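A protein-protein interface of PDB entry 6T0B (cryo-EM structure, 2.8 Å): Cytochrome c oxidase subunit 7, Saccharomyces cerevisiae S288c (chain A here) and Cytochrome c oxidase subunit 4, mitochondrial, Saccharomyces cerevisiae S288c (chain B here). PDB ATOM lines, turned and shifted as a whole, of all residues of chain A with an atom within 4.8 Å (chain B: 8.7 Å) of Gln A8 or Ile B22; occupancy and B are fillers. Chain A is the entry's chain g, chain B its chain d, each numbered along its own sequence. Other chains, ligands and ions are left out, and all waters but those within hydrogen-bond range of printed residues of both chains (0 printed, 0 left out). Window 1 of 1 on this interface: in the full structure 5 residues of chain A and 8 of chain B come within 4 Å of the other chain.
The side-chain amide nitrogen (NE2) of Gln A12 lies within hydrogen-bond range of the side-chain hydroxyl (OG1) of Thr B39 (3.3 Å).
Among the printed residues, merely in contact across the chains: Val A4 with Gln B37 (3.4 Å), Ile A5 with Ile B22 (3.7 Å), Ile A5 with Gly B23 (3.4 Å), Ile A5 with Pro B24 (3.99 Å), Ile A5 with Gly B25 (3.7 Å), Gln A8 with Ile B22 (3.6 Å), Gln A8 with Thr B39 (3.3 Å), Gln A12 with Pro B18 (3.7 Å) and Gln A12 with Ile B22 (3.5 Å).
Gln A8 touches two residues of chain B.
Of chain A, only Ile A5, Gln A8 and Gln A12 come within 4 Å of Ile B22.
Of the printed residues of chain A, Pro B24 touches Ile A5 (3.99 Å).
Printed residues of chain A within 4 Å of Thr B39: Gln A8 (3.3 Å) and Gln A12 (3.3 Å).
The nearest residue of chain B that does not touch Gln A8 is Gln B37 (4.05 Å).
The nearest printed residue of chain A that does not touch Pro B18 is Gln A8 (8.0 Å).
Along chain A the printed residues that touch a printed residue of chain B span positions 4 to 12.
Of the 23 printed residues of chain B, 7 touch a printed residue of chain A.
Among the printed residues, 10 pairs touch across the chains.
Among the printed residues, no Asp or Glu carboxylate lies within 4 Å of a Lys or Arg side-chain nitrogen of the other chain.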
ATOM      1  N   VAL A   4       0.947  17.786  23.795  1.00  0.00           N
ATOM      2  CA  VAL A   4       1.982  16.919  24.339  1.00  0.00           C
ATOM      3  C   VAL A   4       3.048  17.710  25.089  1.00  0.00           C
ATOM      4  O   VAL A   4       3.551  17.247  26.114  1.00  0.00           O
ATOM      5  CB  VAL A   4       2.553  16.048  23.205  1.00  0.00           C
ATOM      6  CG1 VAL A   4       3.059  16.899  22.106  1.00  0.00           C
ATOM      7  CG2 VAL A   4       3.626  15.129  23.691  1.00  0.00           C
ATOM      8  N   ILE A   5       3.345  18.941  24.668  1.00  0.00           N
ATOM      9  CA  ILE A   5       4.293  19.769  25.406  1.00  0.00           C
ATOM     10  C   ILE A   5       3.670  20.251  26.702  1.00  0.00           C
ATOM     11  O   ILE A   5       4.307  20.242  27.764  1.00  0.00           O
ATOM     12  CB  ILE A   5       4.753  20.942  24.531  1.00  0.00           C
ATOM     13  CG1 ILE A   5       5.359  20.428  23.231  1.00  0.00           C
ATOM     14  CG2 ILE A   5       5.730  21.805  25.275  1.00  0.00           C
ATOM     15  CD1 ILE A   5       6.697  19.804  23.379  1.00  0.00           C
ATOM     16  N   GLN A   6       2.394  20.630  26.642  1.00  0.00           N
ATOM     17  CA  GLN A   6       1.662  21.053  27.823  1.00  0.00           C
ATOM     18  C   GLN A   6       1.502  19.922  28.823  1.00  0.00           C
ATOM     19  O   GLN A   6       1.434  20.173  30.028  1.00  0.00           O
ATOM     20  CB  GLN A   6       0.307  21.595  27.401  1.00  0.00           C
ATOM     21  CG  GLN A   6      -0.421  22.357  28.467  1.00  0.00           C
ATOM     22  CD  GLN A   6      -1.703  22.951  27.954  1.00  0.00           C
ATOM     23  OE1 GLN A   6      -2.200  22.559  26.899  1.00  0.00           O
ATOM     24  NE2 GLN A   6      -2.250  23.910  28.690  1.00  0.00           N
ATOM     25  N   LEU A   7       1.476  18.675  28.352  1.00  0.00           N
ATOM     26  CA  LEU A   7       1.384  17.534  29.251  1.00  0.00           C
ATOM     27  C   LEU A   7       2.750  17.105  29.756  1.00  0.00           C
ATOM     28  O   LEU A   7       2.848  16.569  30.865  1.00  0.00           O
ATOM     29  CB  LEU A   7       0.694  16.362  28.556  1.00  0.00           C
ATOM     30  CG  LEU A   7      -0.805  16.151  28.776  1.00  0.00           C
ATOM     31  CD1 LEU A   7      -1.071  15.785  30.206  1.00  0.00           C
ATOM     32  CD2 LEU A   7      -1.633  17.366  28.397  1.00  0.00           C
ATOM     33  N   GLN A   8       3.800  17.319  28.962  1.00  0.00           N
ATOM     34  CA  GLN A   8       5.161  17.116  29.438  1.00  0.00           C
ATOM     35  C   GLN A   8       5.467  18.039  30.597  1.00  0.00           C
ATOM     36  O   GLN A   8       6.048  17.619  31.604  1.00  0.00           O
ATOM     37  CB  GLN A   8       6.151  17.366  28.308  1.00  0.00           C
ATOM     38  CG  GLN A   8       6.432  16.177  27.455  1.00  0.00           C
ATOM     39  CD  GLN A   8       6.963  16.554  26.110  1.00  0.00           C
ATOM     40  OE1 GLN A   8       7.350  17.693  25.892  1.00  0.00           O
ATOM     41  NE2 GLN A   8       7.008  15.602  25.199  1.00  0.00           N
ATOM     42  N   LYS A   9       5.040  19.295  30.489  1.00  0.00           N
ATOM     43  CA  LYS A   9       5.286  20.262  31.546  1.00  0.00           C
ATOM     44  C   LYS A   9       4.497  19.968  32.811  1.00  0.00           C
ATOM     45  O   LYS A   9       4.808  20.536  33.859  1.00  0.00           O
ATOM     46  CB  LYS A   9       4.963  21.665  31.049  1.00  0.00           C
ATOM     47  CG  LYS A   9       5.895  22.145  29.956  1.00  0.00           C
ATOM     48  CD  LYS A   9       5.665  23.595  29.622  1.00  0.00           C
ATOM     49  CE  LYS A   9       4.391  23.780  28.840  1.00  0.00           C
ATOM     50  NZ  LYS A   9       4.209  25.193  28.425  1.00  0.00           N
ATOM     51  N   ILE A  10       3.483  19.111  32.744  1.00  0.00           N
ATOM     52  CA  ILE A  10       2.766  18.670  33.936  1.00  0.00           C
ATOM     53  C   ILE A  10       3.386  17.411  34.509  1.00  0.00           C
ATOM     54  O   ILE A  10       3.607  17.312  35.716  1.00  0.00           O
ATOM     55  CB  ILE A  10       1.275  18.460  33.614  1.00  0.00           C
ATOM     56  CG1 ILE A  10       0.633  19.762  33.155  1.00  0.00           C
ATOM     57  CG2 ILE A  10       0.540  17.940  34.817  1.00  0.00           C
ATOM     58  CD1 ILE A  10       0.647  20.853  34.190  1.00  0.00           C
ATOM     59  N   PHE A  11       3.699  16.445  33.646  1.00  0.00           N
ATOM     60  CA  PHE A  11       4.205  15.157  34.101  1.00  0.00           C
ATOM     61  C   PHE A  11       5.613  15.248  34.651  1.00  0.00           C
ATOM     62  O   PHE A  11       6.007  14.412  35.467  1.00  0.00           O
ATOM     63  CB  PHE A  11       4.199  14.156  32.960  1.00  0.00           C
ATOM     64  CG  PHE A  11       2.934  13.412  32.825  1.00  0.00           C
ATOM     65  CD1 PHE A  11       1.794  14.043  32.404  1.00  0.00           C
ATOM     66  CD2 PHE A  11       2.885  12.077  33.101  1.00  0.00           C
ATOM     67  CE1 PHE A  11       0.637  13.357  32.274  1.00  0.00           C
ATOM     68  CE2 PHE A  11       1.729  11.390  32.971  1.00  0.00           C
ATOM     69  CZ  PHE A  11       0.608  12.023  32.554  1.00  0.00           C
ATOM     70  N   GLN A  12       6.393  16.227  34.210  1.00  0.00           N
ATOM     71  CA  GLN A  12       7.742  16.345  34.736  1.00  0.00           C
ATOM     72  C   GLN A  12       7.792  17.209  35.979  1.00  0.00           C
ATOM     73  O   GLN A  12       8.597  16.955  36.877  1.00  0.00           O
ATOM     74  CB  GLN A  12       8.669  16.908  33.671  1.00  0.00           C
ATOM     75  CG  GLN A  12       8.809  16.004  32.506  1.00  0.00           C
ATOM     76  CD  GLN A  12       9.807  16.509  31.535  1.00  0.00           C
ATOM     77  OE1 GLN A  12      10.584  17.397  31.850  1.00  0.00           O
ATOM     78  NE2 GLN A  12       9.800  15.958  30.339  1.00  0.00           N
ATOM     79  N   SER A  13       6.952  18.229  36.046  1.00  0.00           N
ATOM     80  CA  SER A  13       6.919  19.126  37.193  1.00  0.00           C
ATOM     81  C   SER A  13       5.818  18.718  38.161  1.00  0.00           C
ATOM     82  O   SER A  13       4.929  19.500  38.480  1.00  0.00           O
ATOM     83  CB  SER A  13       6.716  20.559  36.727  1.00  0.00           C
ATOM     84  OG  SER A  13       5.339  20.830  36.578  1.00  0.00           O
ATOM     85  N   VAL B   6      12.046  29.703  30.668  1.00  0.00           N
ATOM     86  CA  VAL B   6      13.173  28.900  30.253  1.00  0.00           C
ATOM     87  C   VAL B   6      13.078  28.673  28.751  1.00  0.00           C
ATOM     88  O   VAL B   6      12.067  28.966  28.118  1.00  0.00           O
ATOM     89  CB  VAL B   6      13.230  27.557  31.004  1.00  0.00           C
ATOM     90  CG1 VAL B   6      13.128  27.789  32.486  1.00  0.00           C
ATOM     91  CG2 VAL B   6      12.119  26.646  30.525  1.00  0.00           C
ATOM     92  N   LYS B   7      14.154  28.165  28.160  1.00  0.00           N
ATOM     93  CA  LYS B   7      14.034  27.750  26.775  1.00  0.00           C
ATOM     94  C   LYS B   7      14.745  26.417  26.553  1.00  0.00           C
ATOM     95  O   LYS B   7      15.115  25.746  27.514  1.00  0.00           O
ATOM     96  CB  LYS B   7      14.497  28.889  25.856  1.00  0.00           C
ATOM     97  CG  LYS B   7      15.945  29.265  25.895  1.00  0.00           C
ATOM     98  CD  LYS B   7      16.680  28.692  24.708  1.00  0.00           C
ATOM     99  CE  LYS B   7      18.144  28.956  24.724  1.00  0.00           C
ATOM    100  NZ  LYS B   7      18.777  28.241  23.593  1.00  0.00           N
ATOM    101  N   THR B   8      14.975  26.053  25.294  1.00  0.00           N
ATOM    102  CA  THR B   8      14.912  24.690  24.799  1.00  0.00           C
ATOM    103  C   THR B   8      16.274  24.028  24.550  1.00  0.00           C
ATOM    104  O   THR B   8      16.307  22.832  24.228  1.00  0.00           O
ATOM    105  CB  THR B   8      14.054  24.735  23.537  1.00  0.00           C
ATOM    106  OG1 THR B   8      12.975  25.653  23.764  1.00  0.00           O
ATOM    107  CG2 THR B   8      13.434  23.431  23.228  1.00  0.00           C
ATOM    108  N   ALA B   9      17.392  24.737  24.758  1.00  0.00           N
ATOM    109  CA  ALA B   9      18.745  24.159  24.738  1.00  0.00           C
ATOM    110  C   ALA B   9      19.077  23.544  23.376  1.00  0.00           C
ATOM    111  O   ALA B   9      18.977  22.334  23.173  1.00  0.00           O
ATOM    112  CB  ALA B   9      18.965  23.139  25.862  1.00  0.00           C
ATOM    113  N   GLY B  17      19.984  21.266  33.558  1.00  0.00           N
ATOM    114  CA  GLY B  17      18.992  20.480  34.241  1.00  0.00           C
ATOM    115  C   GLY B  17      18.019  19.839  33.282  1.00  0.00           C
ATOM    116  O   GLY B  17      18.276  19.749  32.084  1.00  0.00           O
ATOM    117  N   PRO B  18      16.893  19.350  33.797  1.00  0.00           N
ATOM    118  CA  PRO B  18      15.886  18.712  32.944  1.00  0.00           C
ATOM    119  C   PRO B  18      14.724  19.594  32.515  1.00  0.00           C
ATOM    120  O   PRO B  18      13.900  19.135  31.721  1.00  0.00           O
ATOM    121  CB  PRO B  18      15.389  17.589  33.846  1.00  0.00           C
ATOM    122  CG  PRO B  18      15.400  18.211  35.170  1.00  0.00           C
ATOM    123  CD  PRO B  18      16.620  19.089  35.216  1.00  0.00           C
ATOM    124  N   GLU B  19      14.615  20.824  32.997  1.00  0.00           N
ATOM    125  CA  GLU B  19      13.565  21.725  32.544  1.00  0.00           C
ATOM    126  C   GLU B  19      13.935  22.457  31.272  1.00  0.00           C
ATOM    127  O   GLU B  19      13.167  23.308  30.817  1.00  0.00           O
ATOM    128  CB  GLU B  19      13.237  22.746  33.623  1.00  0.00           C
ATOM    129  CG  GLU B  19      12.599  22.147  34.843  1.00  0.00           C
ATOM    130  CD  GLU B  19      12.292  23.185  35.891  1.00  0.00           C
ATOM    131  OE1 GLU B  19      12.714  24.345  35.711  1.00  0.00           O
ATOM    132  OE2 GLU B  19      11.628  22.842  36.891  1.00  0.00           O
ATOM    133  N   THR B  20      15.086  22.153  30.699  1.00  0.00           N
ATOM    134  CA  THR B  20      15.556  22.776  29.483  1.00  0.00           C
ATOM    135  C   THR B  20      15.440  21.850  28.295  1.00  0.00           C
ATOM    136  O   THR B  20      15.771  22.244  27.176  1.00  0.00           O
ATOM    137  CB  THR B  20      17.000  23.190  29.657  1.00  0.00           C
ATOM    138  OG1 THR B  20      17.387  24.013  28.560  1.00  0.00           O
ATOM    139  CG2 THR B  20      17.852  21.964  29.679  1.00  0.00           C
ATOM    140  N   LEU B  21      14.989  20.622  28.516  1.00  0.00           N
ATOM    141  CA  LEU B  21      14.918  19.614  27.470  1.00  0.00           C
ATOM    142  C   LEU B  21      13.495  19.392  27.013  1.00  0.00           C
ATOM    143  O   LEU B  21      13.107  18.257  26.791  1.00  0.00           O
ATOM    144  CB  LEU B  21      15.520  18.306  27.959  1.00  0.00           C
ATOM    145  CG  LEU B  21      16.986  18.287  28.370  1.00  0.00           C
ATOM    146  CD1 LEU B  21      17.187  17.294  29.473  1.00  0.00           C
ATOM    147  CD2 LEU B  21      17.866  17.934  27.207  1.00  0.00           C
ATOM    148  N   ILE B  22      12.682  20.431  26.881  1.00  0.00           N
ATOM    149  CA  ILE B  22      11.261  20.210  26.669  1.00  0.00           C
ATOM    150  C   ILE B  22      10.935  20.093  25.187  1.00  0.00           C
ATOM    151  O   ILE B  22      10.485  19.039  24.726  1.00  0.00           O
ATOM    152  CB  ILE B  22      10.433  21.309  27.348  1.00  0.00           C
ATOM    153  CG1 ILE B  22      10.552  21.171  28.857  1.00  0.00           C
ATOM    154  CG2 ILE B  22       8.976  21.182  26.983  1.00  0.00           C
ATOM    155  CD1 ILE B  22      10.034  19.869  29.385  1.00  0.00           C
ATOM    156  N   GLY B  23      11.159  21.143  24.419  1.00  0.00           N
ATOM    157  CA  GLY B  23      10.804  21.083  23.025  1.00  0.00           C
ATOM    158  C   GLY B  23       9.701  22.043  22.652  1.00  0.00           C
ATOM    159  O   GLY B  23       8.864  22.421  23.474  1.00  0.00           O
ATOM    160  N   PRO B  24       9.697  22.478  21.401  1.00  0.00           N
ATOM    161  CA  PRO B  24       8.503  23.102  20.837  1.00  0.00           C
ATOM    162  C   PRO B  24       7.622  22.041  20.204  1.00  0.00           C
ATOM    163  O   PRO B  24       8.092  21.013  19.726  1.00  0.00           O
ATOM    164  CB  PRO B  24       9.085  24.047  19.782  1.00  0.00           C
ATOM    165  CG  PRO B  24      10.332  23.369  19.338  1.00  0.00           C
ATOM    166  CD  PRO B  24      10.862  22.602  20.512  1.00  0.00           C
ATOM    167  N   GLY B  25       6.328  22.282  20.206  1.00  0.00           N
ATOM    168  CA  GLY B  25       5.430  21.310  19.620  1.00  0.00           C
ATOM    169  C   GLY B  25       5.511  21.292  18.105  1.00  0.00           C
ATOM    170  O   GLY B  25       6.129  22.144  17.471  1.00  0.00           O
ATOM    171  N   ASP B  34      11.748  14.468  15.972  1.00  0.00           N
ATOM    172  CA  ASP B  34      12.111  14.326  17.373  1.00  0.00           C
ATOM    173  C   ASP B  34      12.859  15.516  17.940  1.00  0.00           C
ATOM    174  O   ASP B  34      13.030  15.581  19.155  1.00  0.00           O
ATOM    175  CB  ASP B  34      12.921  13.054  17.590  1.00  0.00           C
ATOM    176  CG  ASP B  34      12.051  11.814  17.677  1.00  0.00           C
ATOM    177  OD1 ASP B  34      10.931  11.890  18.231  1.00  0.00           O
ATOM    178  OD2 ASP B  34      12.484  10.755  17.166  1.00  0.00           O
ATOM    179  N   LEU B  35      13.276  16.473  17.120  1.00  0.00           N
ATOM    180  CA  LEU B  35      13.731  17.725  17.689  1.00  0.00           C
ATOM    181  C   LEU B  35      12.569  18.538  18.221  1.00  0.00           C
ATOM    182  O   LEU B  35      12.784  19.432  19.038  1.00  0.00           O
ATOM    183  CB  LEU B  35      14.518  18.515  16.655  1.00  0.00           C
ATOM    184  CG  LEU B  35      16.001  18.177  16.653  1.00  0.00           C
ATOM    185  CD1 LEU B  35      16.708  18.983  15.599  1.00  0.00           C
ATOM    186  CD2 LEU B  35      16.590  18.452  18.006  1.00  0.00           C
ATOM    187  N   ASP B  36      11.344  18.240  17.791  1.00  0.00           N
ATOM    188  CA  ASP B  36      10.187  18.922  18.347  1.00  0.00           C
ATOM    189  C   ASP B  36       9.767  18.313  19.679  1.00  0.00           C
ATOM    190  O   ASP B  36       9.776  18.983  20.713  1.00  0.00           O
ATOM    191  CB  ASP B  36       9.023  18.885  17.359  1.00  0.00           C
ATOM    192  CG  ASP B  36       9.234  19.793  16.179  1.00  0.00           C
ATOM    193  OD1 ASP B  36       9.179  21.024  16.360  1.00  0.00           O
ATOM    194  OD2 ASP B  36       9.458  19.280  15.067  1.00  0.00           O
ATOM    195  N   GLN B  37       9.422  17.034  19.684  1.00  0.00           N
ATOM    196  CA  GLN B  37       8.733  16.494  20.843  1.00  0.00           C
ATOM    197  C   GLN B  37       9.451  15.345  21.530  1.00  0.00           C
ATOM    198  O   GLN B  37       8.833  14.319  21.823  1.00  0.00           O
ATOM    199  CB  GLN B  37       7.346  16.029  20.440  1.00  0.00           C
ATOM    200  CG  GLN B  37       6.466  17.125  19.952  1.00  0.00           C
ATOM    201  CD  GLN B  37       5.190  16.585  19.434  1.00  0.00           C
ATOM    202  OE1 GLN B  37       4.918  15.403  19.581  1.00  0.00           O
ATOM    203  NE2 GLN B  37       4.379  17.439  18.836  1.00  0.00           N
ATOM    204  N   GLU B  38      10.738  15.490  21.795  1.00  0.00           N
ATOM    205  CA  GLU B  38      11.452  14.551  22.642  1.00  0.00           C
ATOM    206  C   GLU B  38      11.858  15.280  23.905  1.00  0.00           C
ATOM    207  O   GLU B  38      12.115  16.479  23.868  1.00  0.00           O
ATOM    208  CB  GLU B  38      12.677  13.983  21.946  1.00  0.00           C
ATOM    209  CG  GLU B  38      13.259  12.754  22.597  1.00  0.00           C
ATOM    210  CD  GLU B  38      12.304  11.580  22.596  1.00  0.00           C
ATOM    211  OE1 GLU B  38      12.026  11.038  21.507  1.00  0.00           O
ATOM    212  OE2 GLU B  38      11.828  11.198  23.685  1.00  0.00           O
ATOM    213  N   THR B  39      11.858  14.581  25.033  1.00  0.00           N
ATOM    214  CA  THR B  39      12.326  15.166  26.275  1.00  0.00           C
ATOM    215  C   THR B  39      13.280  14.239  26.989  1.00  0.00           C
ATOM    216  O   THR B  39      13.540  13.113  26.562  1.00  0.00           O
ATOM    217  CB  THR B  39      11.212  15.484  27.256  1.00  0.00           C
ATOM    218  OG1 THR B  39      10.482  14.291  27.543  1.00  0.00           O
ATOM    219  CG2 THR B  39      10.316  16.507  26.731  1.00  0.00           C
ATOM    220  N   GLY B  40      13.792  14.767  28.094  1.00  0.00           N
ATOM    221  CA  GLY B  40      14.469  13.970  29.087  1.00  0.00           C
ATOM    222  C   GLY B  40      15.768  13.385  28.592  1.00  0.00           C
ATOM    223  O   GLY B  40      16.526  14.002  27.833  1.00  0.00           O
ATOM    224  N   ARG B  43      16.092  13.026  24.849  1.00  0.00           N
ATOM    225  CA  ARG B  43      16.490  14.247  24.162  1.00  0.00           C
ATOM    226  C   ARG B  43      17.952  14.571  24.399  1.00  0.00           C
ATOM    227  O   ARG B  43      18.614  15.109  23.506  1.00  0.00           O
ATOM    228  CB  ARG B  43      15.631  15.424  24.589  1.00  0.00           C
ATOM    229  CG  ARG B  43      15.737  16.567  23.614  1.00  0.00           C
ATOM    230  CD  ARG B  43      15.057  17.819  24.042  1.00  0.00           C
ATOM    231  NE  ARG B  43      15.198  18.821  23.002  1.00  0.00           N
ATOM    232  CZ  ARG B  43      14.344  18.980  22.005  1.00  0.00           C
ATOM    233  NH1 ARG B  43      13.281  18.212  21.918  1.00  0.00           N
ATOM    234  NH2 ARG B  43      14.555  19.911  21.098  1.00  0.00           N
ATOM    235  N   LEU B  44      18.470  14.244  25.582  1.00  0.00           N
ATOM    236  CA  LEU B  44      19.886  14.448  25.854  1.00  0.00           C
ATOM    237  C   LEU B  44      20.745  13.609  24.928  1.00  0.00           C
ATOM    238  O   LEU B  44      21.714  14.100  24.336  1.00  0.00           O
ATOM    239  CB  LEU B  44      20.176  14.100  27.303  1.00  0.00           C
ATOM    240  CG  LEU B  44      21.452  14.667  27.887  1.00  0.00           C
ATOM    241  CD1 LEU B  44      21.421  16.166  27.851  1.00  0.00           C
ATOM    242  CD2 LEU B  44      21.585  14.177  29.292  1.00  0.00           C
ATOM    243  N   LEU B  47      20.524  15.027  21.344  1.00  0.00           N
ATOM    244  CA  LEU B  47      21.379  16.203  21.202  1.00  0.00           C
ATOM    245  C   LEU B  47      22.842  15.816  21.077  1.00  0.00           C
ATOM    246  O   LEU B  47      23.578  16.371  20.247  1.00  0.00           O
ATOM    247  CB  LEU B  47      21.203  17.119  22.405  1.00  0.00           C
ATOM    248  CG  LEU B  47      19.994  18.019  22.404  1.00  0.00           C
ATOM    249  CD1 LEU B  47      20.053  18.895  23.613  1.00  0.00           C
ATOM    250  CD2 LEU B  47      20.013  18.839  21.157  1.00  0.00           C
